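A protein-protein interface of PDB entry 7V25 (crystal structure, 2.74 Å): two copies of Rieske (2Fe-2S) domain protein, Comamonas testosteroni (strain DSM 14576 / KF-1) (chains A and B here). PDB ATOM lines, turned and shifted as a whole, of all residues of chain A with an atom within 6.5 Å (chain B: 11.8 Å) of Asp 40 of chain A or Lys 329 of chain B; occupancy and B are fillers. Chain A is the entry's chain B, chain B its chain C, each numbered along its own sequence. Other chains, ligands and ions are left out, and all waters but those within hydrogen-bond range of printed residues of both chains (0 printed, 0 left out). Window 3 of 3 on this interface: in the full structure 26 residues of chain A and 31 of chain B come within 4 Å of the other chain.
OD2 of Asp 40 of chain A lies within hydrogen-bond range of OG of Ser 59 of chain A (2.7 Å).
ND2 of Asn 82 of chain A is in hydrogen-bond range of O of Arg 57 of chain A (2.9 Å).
The side-chain carboxylate (OE1) of Glu 83 of chain A lies within salt-bridge range of the guanidinium group (NE) of Arg 81 of chain A, at 2.8 Å.
O of Gly 86 of chain A lies close to OD1 of Asn 82 of chain A.
The guanidinium group (NE) of Arg 325 of chain B sits close to the side-chain sulfur (SD) of Met 328 of chain B (3.5 Å).
The backbone NH (N) of Gly 335 of chain B is in hydrogen-bond range of the side-chain amide oxygen (OD1) of Asn 332 of chain B (2.9 Å).
The backbone carbonyl oxygen of Asp 40 of chain A lies within hydrogen-bond range of the side-chain amino group of Lys 329 of chain B.
The guanidinium group of Arg 81 of chain A is in hydrogen-bond range of the backbone carbonyl oxygen of Met 328 of chain B (3.1 Å).
NH1 of Arg 81 of chain A lies within hydrogen-bond range of O of Asn 332 of chain B, at 2.9 Å.
O of Phe 333 of chain B sits at hydrogen-bond distance from NH1 of Arg 81 of chain A (2.9 Å).
No residue of chain B comes within 4 Å of Gly 41 of chain A.
Printed residues of chain B within 4 Å of Pro 43 of chain A: Arg 325.
No residue of chain B comes within 4 Å of Ser 59 of chain A.
Printed residues of chain B within 4 Å of Arg 81 of chain A: Met 328, Asn 332 and Phe 333.
Asn 82 of chain A touches just one residue of chain B: Lys 329 (3.9 Å).
No residue of chain B comes within 4 Å of Glu 83 of chain A.
Gly 86 of chain A touches none of the printed residues of chain B.
Trp 322 of chain B touches none of the printed residues of chain A.
Of the printed residues of chain A, Arg 325 of chain B touches Thr 42 (3.6 Å) and Pro 43 (3.5 Å).
Asn 326 of chain B touches none of the printed residues of chain A.
Of the printed residues of chain A, Met 328 of chain B touches Arg 81.
Lys 329 of chain B touches just these residues of chain A: Asp 40 and Asn 82.
Printed residues of chain A within 4 Å of Asn 332 of chain B: Arg 81 (2.9 Å).
No position is printed for both chains.
Hydrophobic or aromatic side chains of chain A within 4 Å of the printed part of chain B: Pro 43.
Among the printed residues, 7 pairs touch across the chains.
Among the printed residues, no Asp or Glu carboxylate lies within 4 Å of a Lys or Arg side-chain nitrogen of the other chain.
Among the printed residues, merely in contact across the chains: Thr 42 of chain A with Arg 325 of chain B, Pro 43 of chain A with Arg 325 of chain B and Asn 82 of chain A with Lys 329 of chain B.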
ATOM      1  N   VAL A  36      -5.673   9.972  35.227  1.00  0.00           N
ATOM      2  CA  VAL A  36      -5.834   9.457  33.874  1.00  0.00           C
ATOM      3  C   VAL A  36      -6.919  10.245  33.146  1.00  0.00           C
ATOM      4  O   VAL A  36      -6.910  10.328  31.912  1.00  0.00           O
ATOM      5  CB  VAL A  36      -6.118   7.948  33.853  1.00  0.00           C
ATOM      6  CG1 VAL A  36      -5.027   7.168  34.544  1.00  0.00           C
ATOM      7  CG2 VAL A  36      -7.465   7.629  34.471  1.00  0.00           C
ATOM      8  N   GLU A  38     -10.447  12.087  31.764  1.00  0.00           N
ATOM      9  CA  GLU A  38     -11.530  11.737  30.859  1.00  0.00           C
ATOM     10  C   GLU A  38     -11.074  10.652  29.883  1.00  0.00           C
ATOM     11  O   GLU A  38      -9.874  10.424  29.714  1.00  0.00           O
ATOM     12  CB  GLU A  38     -12.034  12.979  30.111  1.00  0.00           C
ATOM     13  CG  GLU A  38     -12.860  13.938  30.963  1.00  0.00           C
ATOM     14  CD  GLU A  38     -13.686  13.266  32.053  1.00  0.00           C
ATOM     15  OE1 GLU A  38     -13.242  13.282  33.218  1.00  0.00           O
ATOM     16  OE2 GLU A  38     -14.765  12.712  31.736  1.00  0.00           O
ATOM     17  N   PRO A  39     -12.026   9.960  29.211  1.00  0.00           N
ATOM     18  CA  PRO A  39     -11.693   9.070  28.094  1.00  0.00           C
ATOM     19  C   PRO A  39     -10.876   9.842  27.063  1.00  0.00           C
ATOM     20  O   PRO A  39     -11.061  11.058  26.894  1.00  0.00           O
ATOM     21  CB  PRO A  39     -13.068   8.759  27.490  1.00  0.00           C
ATOM     22  CG  PRO A  39     -14.018   8.887  28.665  1.00  0.00           C
ATOM     23  CD  PRO A  39     -13.474  10.036  29.482  1.00  0.00           C
ATOM     24  N   ASP A  40      -9.952   9.135  26.395  1.00  0.00           N
ATOM     25  CA  ASP A  40      -9.058   9.756  25.426  1.00  0.00           C
ATOM     26  C   ASP A  40      -8.256  10.879  26.082  1.00  0.00           C
ATOM     27  O   ASP A  40      -7.889  11.846  25.417  1.00  0.00           O
ATOM     28  CB  ASP A  40      -9.831  10.306  24.224  1.00  0.00           C
ATOM     29  CG  ASP A  40     -10.488   9.243  23.357  1.00  0.00           C
ATOM     30  OD1 ASP A  40     -11.500   9.570  22.695  1.00  0.00           O
ATOM     31  OD2 ASP A  40      -9.971   8.096  23.342  1.00  0.00           O
ATOM     32  N   GLY A  41      -8.008  10.752  27.391  1.00  0.00           N
ATOM     33  CA  GLY A  41      -7.235  11.722  28.146  1.00  0.00           C
ATOM     34  C   GLY A  41      -5.724  11.572  27.940  1.00  0.00           C
ATOM     35  O   GLY A  41      -5.233  10.529  27.489  1.00  0.00           O
ATOM     36  N   THR A  42      -4.989  12.639  28.283  1.00  0.00           N
ATOM     37  CA  THR A  42      -3.537  12.611  28.288  1.00  0.00           C
ATOM     38  C   THR A  42      -3.013  11.355  28.983  1.00  0.00           C
ATOM     39  O   THR A  42      -3.381  11.069  30.125  1.00  0.00           O
ATOM     40  CB  THR A  42      -3.006  13.822  29.050  1.00  0.00           C
ATOM     41  OG1 THR A  42      -3.725  14.900  28.466  1.00  0.00           O
ATOM     42  CG2 THR A  42      -1.518  14.013  28.875  1.00  0.00           C
ATOM     43  N   PRO A  43      -2.124  10.591  28.312  1.00  0.00           N
ATOM     44  CA  PRO A  43      -1.433   9.446  28.912  1.00  0.00           C
ATOM     45  C   PRO A  43      -0.436   9.839  29.999  1.00  0.00           C
ATOM     46  O   PRO A  43       0.200  10.884  29.930  1.00  0.00           O
ATOM     47  CB  PRO A  43      -0.588   8.877  27.760  1.00  0.00           C
ATOM     48  CG  PRO A  43      -1.225   9.430  26.512  1.00  0.00           C
ATOM     49  CD  PRO A  43      -1.733  10.804  26.911  1.00  0.00           C
ATOM     50  N   ARG A  57      -6.708   6.048  29.692  1.00  0.00           N
ATOM     51  CA  ARG A  57      -8.092   5.641  29.567  1.00  0.00           C
ATOM     52  C   ARG A  57      -8.485   5.718  28.099  1.00  0.00           C
ATOM     53  O   ARG A  57      -8.353   6.778  27.490  1.00  0.00           O
ATOM     54  CB  ARG A  57      -8.990   6.553  30.404  1.00  0.00           C
ATOM     55  CG  ARG A  57     -10.464   6.204  30.264  1.00  0.00           C
ATOM     56  CD  ARG A  57     -11.436   6.898  31.198  1.00  0.00           C
ATOM     57  NE  ARG A  57     -11.018   7.094  32.583  1.00  0.00           N
ATOM     58  CZ  ARG A  57     -11.240   6.250  33.593  1.00  0.00           C
ATOM     59  NH1 ARG A  57     -11.862   5.101  33.391  1.00  0.00           N
ATOM     60  NH2 ARG A  57     -10.828   6.566  34.809  1.00  0.00           N
ATOM     61  N   ASP A  58      -8.974   4.612  27.528  1.00  0.00           N
ATOM     62  CA  ASP A  58      -9.221   4.620  26.093  1.00  0.00           C
ATOM     63  C   ASP A  58     -10.542   5.324  25.793  1.00  0.00           C
ATOM     64  O   ASP A  58     -11.083   5.985  26.669  1.00  0.00           O
ATOM     65  CB  ASP A  58      -8.921   3.271  25.431  1.00  0.00           C
ATOM     66  CG  ASP A  58      -9.985   2.181  25.525  1.00  0.00           C
ATOM     67  OD1 ASP A  58     -11.065   2.416  26.155  1.00  0.00           O
ATOM     68  OD2 ASP A  58      -9.714   1.078  24.954  1.00  0.00           O
ATOM     69  N   SER A  59     -11.043   5.196  24.558  1.00  0.00           N
ATOM     70  CA  SER A  59     -12.247   5.910  24.136  1.00  0.00           C
ATOM     71  C   SER A  59     -13.480   5.395  24.870  1.00  0.00           C
ATOM     72  O   SER A  59     -14.388   6.176  25.119  1.00  0.00           O
ATOM     73  CB  SER A  59     -12.478   5.868  22.642  1.00  0.00           C
ATOM     74  OG  SER A  59     -11.351   6.324  21.920  1.00  0.00           O
ATOM     75  N   GLU A  60     -13.503   4.089  25.186  1.00  0.00           N
ATOM     76  CA  GLU A  60     -14.640   3.436  25.828  1.00  0.00           C
ATOM     77  C   GLU A  60     -14.582   3.662  27.334  1.00  0.00           C
ATOM     78  O   GLU A  60     -15.462   3.229  28.068  1.00  0.00           O
ATOM     79  CB  GLU A  60     -14.678   1.928  25.570  1.00  0.00           C
ATOM     80  CG  GLU A  60     -13.847   1.468  24.383  1.00  0.00           C
ATOM     81  CD  GLU A  60     -14.555   1.326  23.047  1.00  0.00           C
ATOM     82  OE1 GLU A  60     -15.587   0.622  22.997  1.00  0.00           O
ATOM     83  OE2 GLU A  60     -14.061   1.913  22.053  1.00  0.00           O
ATOM     84  N   GLY A  61     -13.522   4.325  27.789  1.00  0.00           N
ATOM     85  CA  GLY A  61     -13.402   4.621  29.201  1.00  0.00           C
ATOM     86  C   GLY A  61     -12.700   3.506  29.972  1.00  0.00           C
ATOM     87  O   GLY A  61     -12.567   3.596  31.198  1.00  0.00           O
ATOM     88  N   ARG A  81      -0.988   9.317  20.695  1.00  0.00           N
ATOM     89  CA  ARG A  81      -2.332   9.860  20.598  1.00  0.00           C
ATOM     90  C   ARG A  81      -3.319   8.840  21.147  1.00  0.00           C
ATOM     91  O   ARG A  81      -3.293   7.670  20.774  1.00  0.00           O
ATOM     92  CB  ARG A  81      -2.688  10.191  19.148  1.00  0.00           C
ATOM     93  CG  ARG A  81      -1.709  11.130  18.456  1.00  0.00           C
ATOM     94  CD  ARG A  81      -2.159  11.451  17.041  1.00  0.00           C
ATOM     95  NE  ARG A  81      -3.509  11.996  17.037  1.00  0.00           N
ATOM     96  CZ  ARG A  81      -3.773  13.287  17.171  1.00  0.00           C
ATOM     97  NH1 ARG A  81      -2.776  14.150  17.276  1.00  0.00           N
ATOM     98  NH2 ARG A  81      -5.028  13.708  17.185  1.00  0.00           N
ATOM     99  N   ASN A  82      -4.184   9.306  22.042  1.00  0.00           N
ATOM    100  CA  ASN A  82      -5.118   8.433  22.724  1.00  0.00           C
ATOM    101  C   ASN A  82      -6.490   8.740  22.158  1.00  0.00           C
ATOM    102  O   ASN A  82      -7.069   9.768  22.489  1.00  0.00           O
ATOM    103  CB  ASN A  82      -5.040   8.640  24.238  1.00  0.00           C
ATOM    104  CG  ASN A  82      -6.060   7.878  25.059  1.00  0.00           C
ATOM    105  OD1 ASN A  82      -6.578   6.834  24.654  1.00  0.00           O
ATOM    106  ND2 ASN A  82      -6.339   8.396  26.246  1.00  0.00           N
ATOM    107  N   GLU A  83      -6.987   7.858  21.283  1.00  0.00           N
ATOM    108  CA  GLU A  83      -8.187   8.197  20.537  1.00  0.00           C
ATOM    109  C   GLU A  83      -8.627   7.011  19.690  1.00  0.00           C
ATOM    110  O   GLU A  83      -7.805   6.214  19.230  1.00  0.00           O
ATOM    111  CB  GLU A  83      -7.909   9.409  19.642  1.00  0.00           C
ATOM    112  CG  GLU A  83      -6.874   9.128  18.568  1.00  0.00           C
ATOM    113  CD  GLU A  83      -6.357  10.326  17.795  1.00  0.00           C
ATOM    114  OE1 GLU A  83      -5.568  10.108  16.841  1.00  0.00           O
ATOM    115  OE2 GLU A  83      -6.734  11.469  18.148  1.00  0.00           O
ATOM    116  N   GLU A  84      -9.938   6.945  19.459  1.00  0.00           N
ATOM    117  CA  GLU A  84     -10.508   5.906  18.625  1.00  0.00           C
ATOM    118  C   GLU A  84     -10.089   4.545  19.176  1.00  0.00           C
ATOM    119  O   GLU A  84      -9.649   3.670  18.427  1.00  0.00           O
ATOM    120  CB  GLU A  84     -10.062   6.081  17.171  1.00  0.00           C
ATOM    121  CG  GLU A  84     -10.510   7.390  16.547  1.00  0.00           C
ATOM    122  CD  GLU A  84      -9.916   7.680  15.177  1.00  0.00           C
ATOM    123  OE1 GLU A  84      -9.087   6.880  14.673  1.00  0.00           O
ATOM    124  OE2 GLU A  84     -10.274   8.716  14.617  1.00  0.00           O
ATOM    125  N   GLY A  85     -10.186   4.422  20.507  1.00  0.00           N
ATOM    126  CA  GLY A  85     -10.067   3.160  21.222  1.00  0.00           C
ATOM    127  C   GLY A  85      -8.634   2.642  21.331  1.00  0.00           C
ATOM    128  O   GLY A  85      -8.416   1.435  21.439  1.00  0.00           O
ATOM    129  N   GLY A  86      -7.655   3.554  21.354  1.00  0.00           N
ATOM    130  CA  GLY A  86      -6.295   3.067  21.386  1.00  0.00           C
ATOM    131  C   GLY A  86      -5.279   4.143  21.720  1.00  0.00           C
ATOM    132  O   GLY A  86      -5.629   5.295  22.006  1.00  0.00           O
ATOM    133  N   SER B 188       1.836  16.365  10.231  1.00  0.00           N
ATOM    134  CA  SER B 188       1.176  17.648  10.419  1.00  0.00           C
ATOM    135  C   SER B 188       2.030  18.786   9.874  1.00  0.00           C
ATOM    136  O   SER B 188       1.577  19.930   9.839  1.00  0.00           O
ATOM    137  CB  SER B 188       0.830  17.883  11.855  1.00  0.00           C
ATOM    138  OG  SER B 188      -0.435  17.326  12.159  1.00  0.00           O
ATOM    139  N   TRP B 322       7.782  20.114  25.353  1.00  0.00           N
ATOM    140  CA  TRP B 322       6.753  21.140  25.217  1.00  0.00           C
ATOM    141  C   TRP B 322       5.532  20.584  24.487  1.00  0.00           C
ATOM    142  O   TRP B 322       4.794  21.334  23.833  1.00  0.00           O
ATOM    143  CB  TRP B 322       7.281  22.448  24.573  1.00  0.00           C
ATOM    144  CG  TRP B 322       8.408  23.132  25.302  1.00  0.00           C
ATOM    145  CD1 TRP B 322       8.765  22.990  26.618  1.00  0.00           C
ATOM    146  CD2 TRP B 322       9.323  24.099  24.754  1.00  0.00           C
ATOM    147  NE1 TRP B 322       9.847  23.772  26.912  1.00  0.00           N
ATOM    148  CE2 TRP B 322      10.209  24.468  25.792  1.00  0.00           C
ATOM    149  CE3 TRP B 322       9.482  24.686  23.493  1.00  0.00           C
ATOM    150  CZ2 TRP B 322      11.216  25.412  25.609  1.00  0.00           C
ATOM    151  CZ3 TRP B 322      10.501  25.591  23.302  1.00  0.00           C
ATOM    152  CH2 TRP B 322      11.349  25.954  24.350  1.00  0.00           C
ATOM    153  N   GLN B 323       5.308  19.270  24.628  1.00  0.00           N
ATOM    154  CA  GLN B 323       4.169  18.655  23.966  1.00  0.00           C
ATOM    155  C   GLN B 323       2.897  19.359  24.413  1.00  0.00           C
ATOM    156  O   GLN B 323       2.596  19.430  25.598  1.00  0.00           O
ATOM    157  CB  GLN B 323       4.095  17.146  24.186  1.00  0.00           C
ATOM    158  CG  GLN B 323       2.927  16.505  23.453  1.00  0.00           C
ATOM    159  CD  GLN B 323       3.044  15.001  23.367  1.00  0.00           C
ATOM    160  OE1 GLN B 323       3.043  14.293  24.372  1.00  0.00           O
ATOM    161  NE2 GLN B 323       3.115  14.489  22.145  1.00  0.00           N
ATOM    162  N   ASP B 324       2.180  19.903  23.436  1.00  0.00           N
ATOM    163  CA  ASP B 324       0.952  20.621  23.716  1.00  0.00           C
ATOM    164  C   ASP B 324      -0.253  19.703  23.480  1.00  0.00           C
ATOM    165  O   ASP B 324      -0.642  19.443  22.341  1.00  0.00           O
ATOM    166  CB  ASP B 324       0.916  21.897  22.885  1.00  0.00           C
ATOM    167  CG  ASP B 324      -0.204  22.831  23.286  1.00  0.00           C
ATOM    168  OD1 ASP B 324      -1.316  22.334  23.568  1.00  0.00           O
ATOM    169  OD2 ASP B 324       0.049  24.060  23.309  1.00  0.00           O
ATOM    170  N   ARG B 325      -0.867  19.231  24.572  1.00  0.00           N
ATOM    171  CA  ARG B 325      -1.898  18.207  24.494  1.00  0.00           C
ATOM    172  C   ARG B 325      -3.170  18.762  23.855  1.00  0.00           C
ATOM    173  O   ARG B 325      -3.928  18.028  23.224  1.00  0.00           O
ATOM    174  CB  ARG B 325      -2.162  17.611  25.880  1.00  0.00           C
ATOM    175  CG  ARG B 325      -1.205  16.494  26.254  1.00  0.00           C
ATOM    176  CD  ARG B 325      -1.567  15.278  25.429  1.00  0.00           C
ATOM    177  NE  ARG B 325      -0.413  14.486  25.029  1.00  0.00           N
ATOM    178  CZ  ARG B 325      -0.508  13.324  24.391  1.00  0.00           C
ATOM    179  NH1 ARG B 325      -1.701  12.839  24.067  1.00  0.00           N
ATOM    180  NH2 ARG B 325       0.594  12.667  24.058  1.00  0.00           N
ATOM    181  N   ASN B 326      -3.394  20.067  24.026  1.00  0.00           N
ATOM    182  CA  ASN B 326      -4.556  20.725  23.449  1.00  0.00           C
ATOM    183  C   ASN B 326      -4.415  20.843  21.935  1.00  0.00           C
ATOM    184  O   ASN B 326      -5.386  20.629  21.213  1.00  0.00           O
ATOM    185  CB  ASN B 326      -4.827  22.079  24.093  1.00  0.00           C
ATOM    186  CG  ASN B 326      -5.445  21.924  25.460  1.00  0.00           C
ATOM    187  OD1 ASN B 326      -6.336  21.104  25.635  1.00  0.00           O
ATOM    188  ND2 ASN B 326      -4.984  22.701  26.425  1.00  0.00           N
ATOM    189  N   ALA B 327      -3.209  21.164  21.455  1.00  0.00           N
ATOM    190  CA  ALA B 327      -2.975  21.236  20.020  1.00  0.00           C
ATOM    191  C   ALA B 327      -3.173  19.859  19.389  1.00  0.00           C
ATOM    192  O   ALA B 327      -3.611  19.767  18.244  1.00  0.00           O
ATOM    193  CB  ALA B 327      -1.596  21.782  19.733  1.00  0.00           C
ATOM    194  N   MET B 328      -2.875  18.796  20.157  1.00  0.00           N
ATOM    195  CA  MET B 328      -3.059  17.439  19.682  1.00  0.00           C
ATOM    196  C   MET B 328      -4.539  17.110  19.539  1.00  0.00           C
ATOM    197  O   MET B 328      -4.915  16.435  18.583  1.00  0.00           O
ATOM    198  CB  MET B 328      -2.401  16.438  20.616  1.00  0.00           C
ATOM    199  CG  MET B 328      -0.912  16.428  20.449  1.00  0.00           C
ATOM    200  SD  MET B 328      -0.135  15.345  21.657  1.00  0.00           S
ATOM    201  CE  MET B 328      -0.313  13.766  20.823  1.00  0.00           C
ATOM    202  N   LYS B 329      -5.367  17.589  20.479  1.00  0.00           N
ATOM    203  CA  LYS B 329      -6.811  17.476  20.320  1.00  0.00           C
ATOM    204  C   LYS B 329      -7.257  18.304  19.116  1.00  0.00           C
ATOM    205  O   LYS B 329      -8.178  17.899  18.420  1.00  0.00           O
ATOM    206  CB  LYS B 329      -7.589  17.940  21.555  1.00  0.00           C
ATOM    207  CG  LYS B 329      -7.623  16.996  22.749  1.00  0.00           C
ATOM    208  CD  LYS B 329      -8.534  15.790  22.618  1.00  0.00           C
ATOM    209  CE  LYS B 329      -8.107  14.644  23.520  1.00  0.00           C
ATOM    210  NZ  LYS B 329      -8.630  13.337  23.056  1.00  0.00           N
ATOM    211  N   ALA B 330      -6.606  19.452  18.865  1.00  0.00           N
ATOM    212  CA  ALA B 330      -6.984  20.302  17.747  1.00  0.00           C
ATOM    213  C   ALA B 330      -6.685  19.615  16.413  1.00  0.00           C
ATOM    214  O   ALA B 330      -7.294  19.958  15.403  1.00  0.00           O
ATOM    215  CB  ALA B 330      -6.384  21.690  17.845  1.00  0.00           C
ATOM    216  N   GLY B 331      -5.779  18.631  16.402  1.00  0.00           N
ATOM    217  CA  GLY B 331      -5.567  17.852  15.189  1.00  0.00           C
ATOM    218  C   GLY B 331      -4.146  17.980  14.641  1.00  0.00           C
ATOM    219  O   GLY B 331      -3.827  17.493  13.557  1.00  0.00           O
ATOM    220  N   ASN B 332      -3.305  18.681  15.394  1.00  0.00           N
ATOM    221  CA  ASN B 332      -1.867  18.615  15.230  1.00  0.00           C
ATOM    222  C   ASN B 332      -1.423  17.241  15.727  1.00  0.00           C
ATOM    223  O   ASN B 332      -1.809  16.834  16.822  1.00  0.00           O
ATOM    224  CB  ASN B 332      -1.226  19.732  16.055  1.00  0.00           C
ATOM    225  CG  ASN B 332       0.195  20.003  15.636  1.00  0.00           C
ATOM    226  OD1 ASN B 332       1.140  19.482  16.232  1.00  0.00           O
ATOM    227  ND2 ASN B 332       0.340  20.785  14.583  1.00  0.00           N
ATOM    228  N   PHE B 333      -0.605  16.530  14.937  1.00  0.00           N
ATOM    229  CA  PHE B 333      -0.267  15.140  15.227  1.00  0.00           C
ATOM    230  C   PHE B 333       0.536  15.008  16.529  1.00  0.00           C
ATOM    231  O   PHE B 333       0.107  14.305  17.443  1.00  0.00           O
ATOM    232  CB  PHE B 333       0.411  14.481  14.024  1.00  0.00           C
ATOM    233  CG  PHE B 333       0.510  12.983  14.109  1.00  0.00           C
ATOM    234  CD1 PHE B 333      -0.615  12.188  13.941  1.00  0.00           C
ATOM    235  CD2 PHE B 333       1.724  12.366  14.358  1.00  0.00           C
ATOM    236  CE1 PHE B 333      -0.526  10.806  14.024  1.00  0.00           C
ATOM    237  CE2 PHE B 333       1.817  10.983  14.448  1.00  0.00           C
ATOM    238  CZ  PHE B 333       0.694  10.206  14.262  1.00  0.00           C
ATOM    239  N   THR B 334       1.683  15.696  16.624  1.00  0.00           N
ATOM    240  CA  THR B 334       2.593  15.508  17.749  1.00  0.00           C
ATOM    241  C   THR B 334       2.439  16.589  18.829  1.00  0.00           C
ATOM    242  O   THR B 334       2.874  16.396  19.967  1.00  0.00           O
ATOM    243  CB  THR B 334       4.060  15.479  17.298  1.00  0.00           C
ATOM    244  OG1 THR B 334       4.476  16.834  17.100  1.00  0.00           O
ATOM    245  CG2 THR B 334       4.322  14.631  16.072  1.00  0.00           C
ATOM    246  N   GLY B 335       1.880  17.750  18.465  1.00  0.00           N
ATOM    247  CA  GLY B 335       1.836  18.879  19.376  1.00  0.00           C
ATOM    248  C   GLY B 335       3.235  19.334  19.795  1.00  0.00           C
ATOM    249  O   GLY B 335       3.391  19.949  20.862  1.00  0.00           O
ATOM    250  N   ILE B 336       4.243  19.035  18.948  1.00  0.00           N
ATOM    251  CA  ILE B 336       5.604  19.498  19.174  1.00  0.00           C
ATOM    252  C   ILE B 336       6.002  20.421  18.027  1.00  0.00           C
ATOM    253  O   ILE B 336       5.771  20.111  16.872  1.00  0.00           O
ATOM    254  CB  ILE B 336       6.569  18.311  19.387  1.00  0.00           C
ATOM    255  CG1 ILE B 336       6.321  17.622  20.730  1.00  0.00           C
ATOM    256  CG2 ILE B 336       8.022  18.749  19.260  1.00  0.00           C
ATOM    257  CD1 ILE B 336       6.611  16.148  20.723  1.00  0.00           C
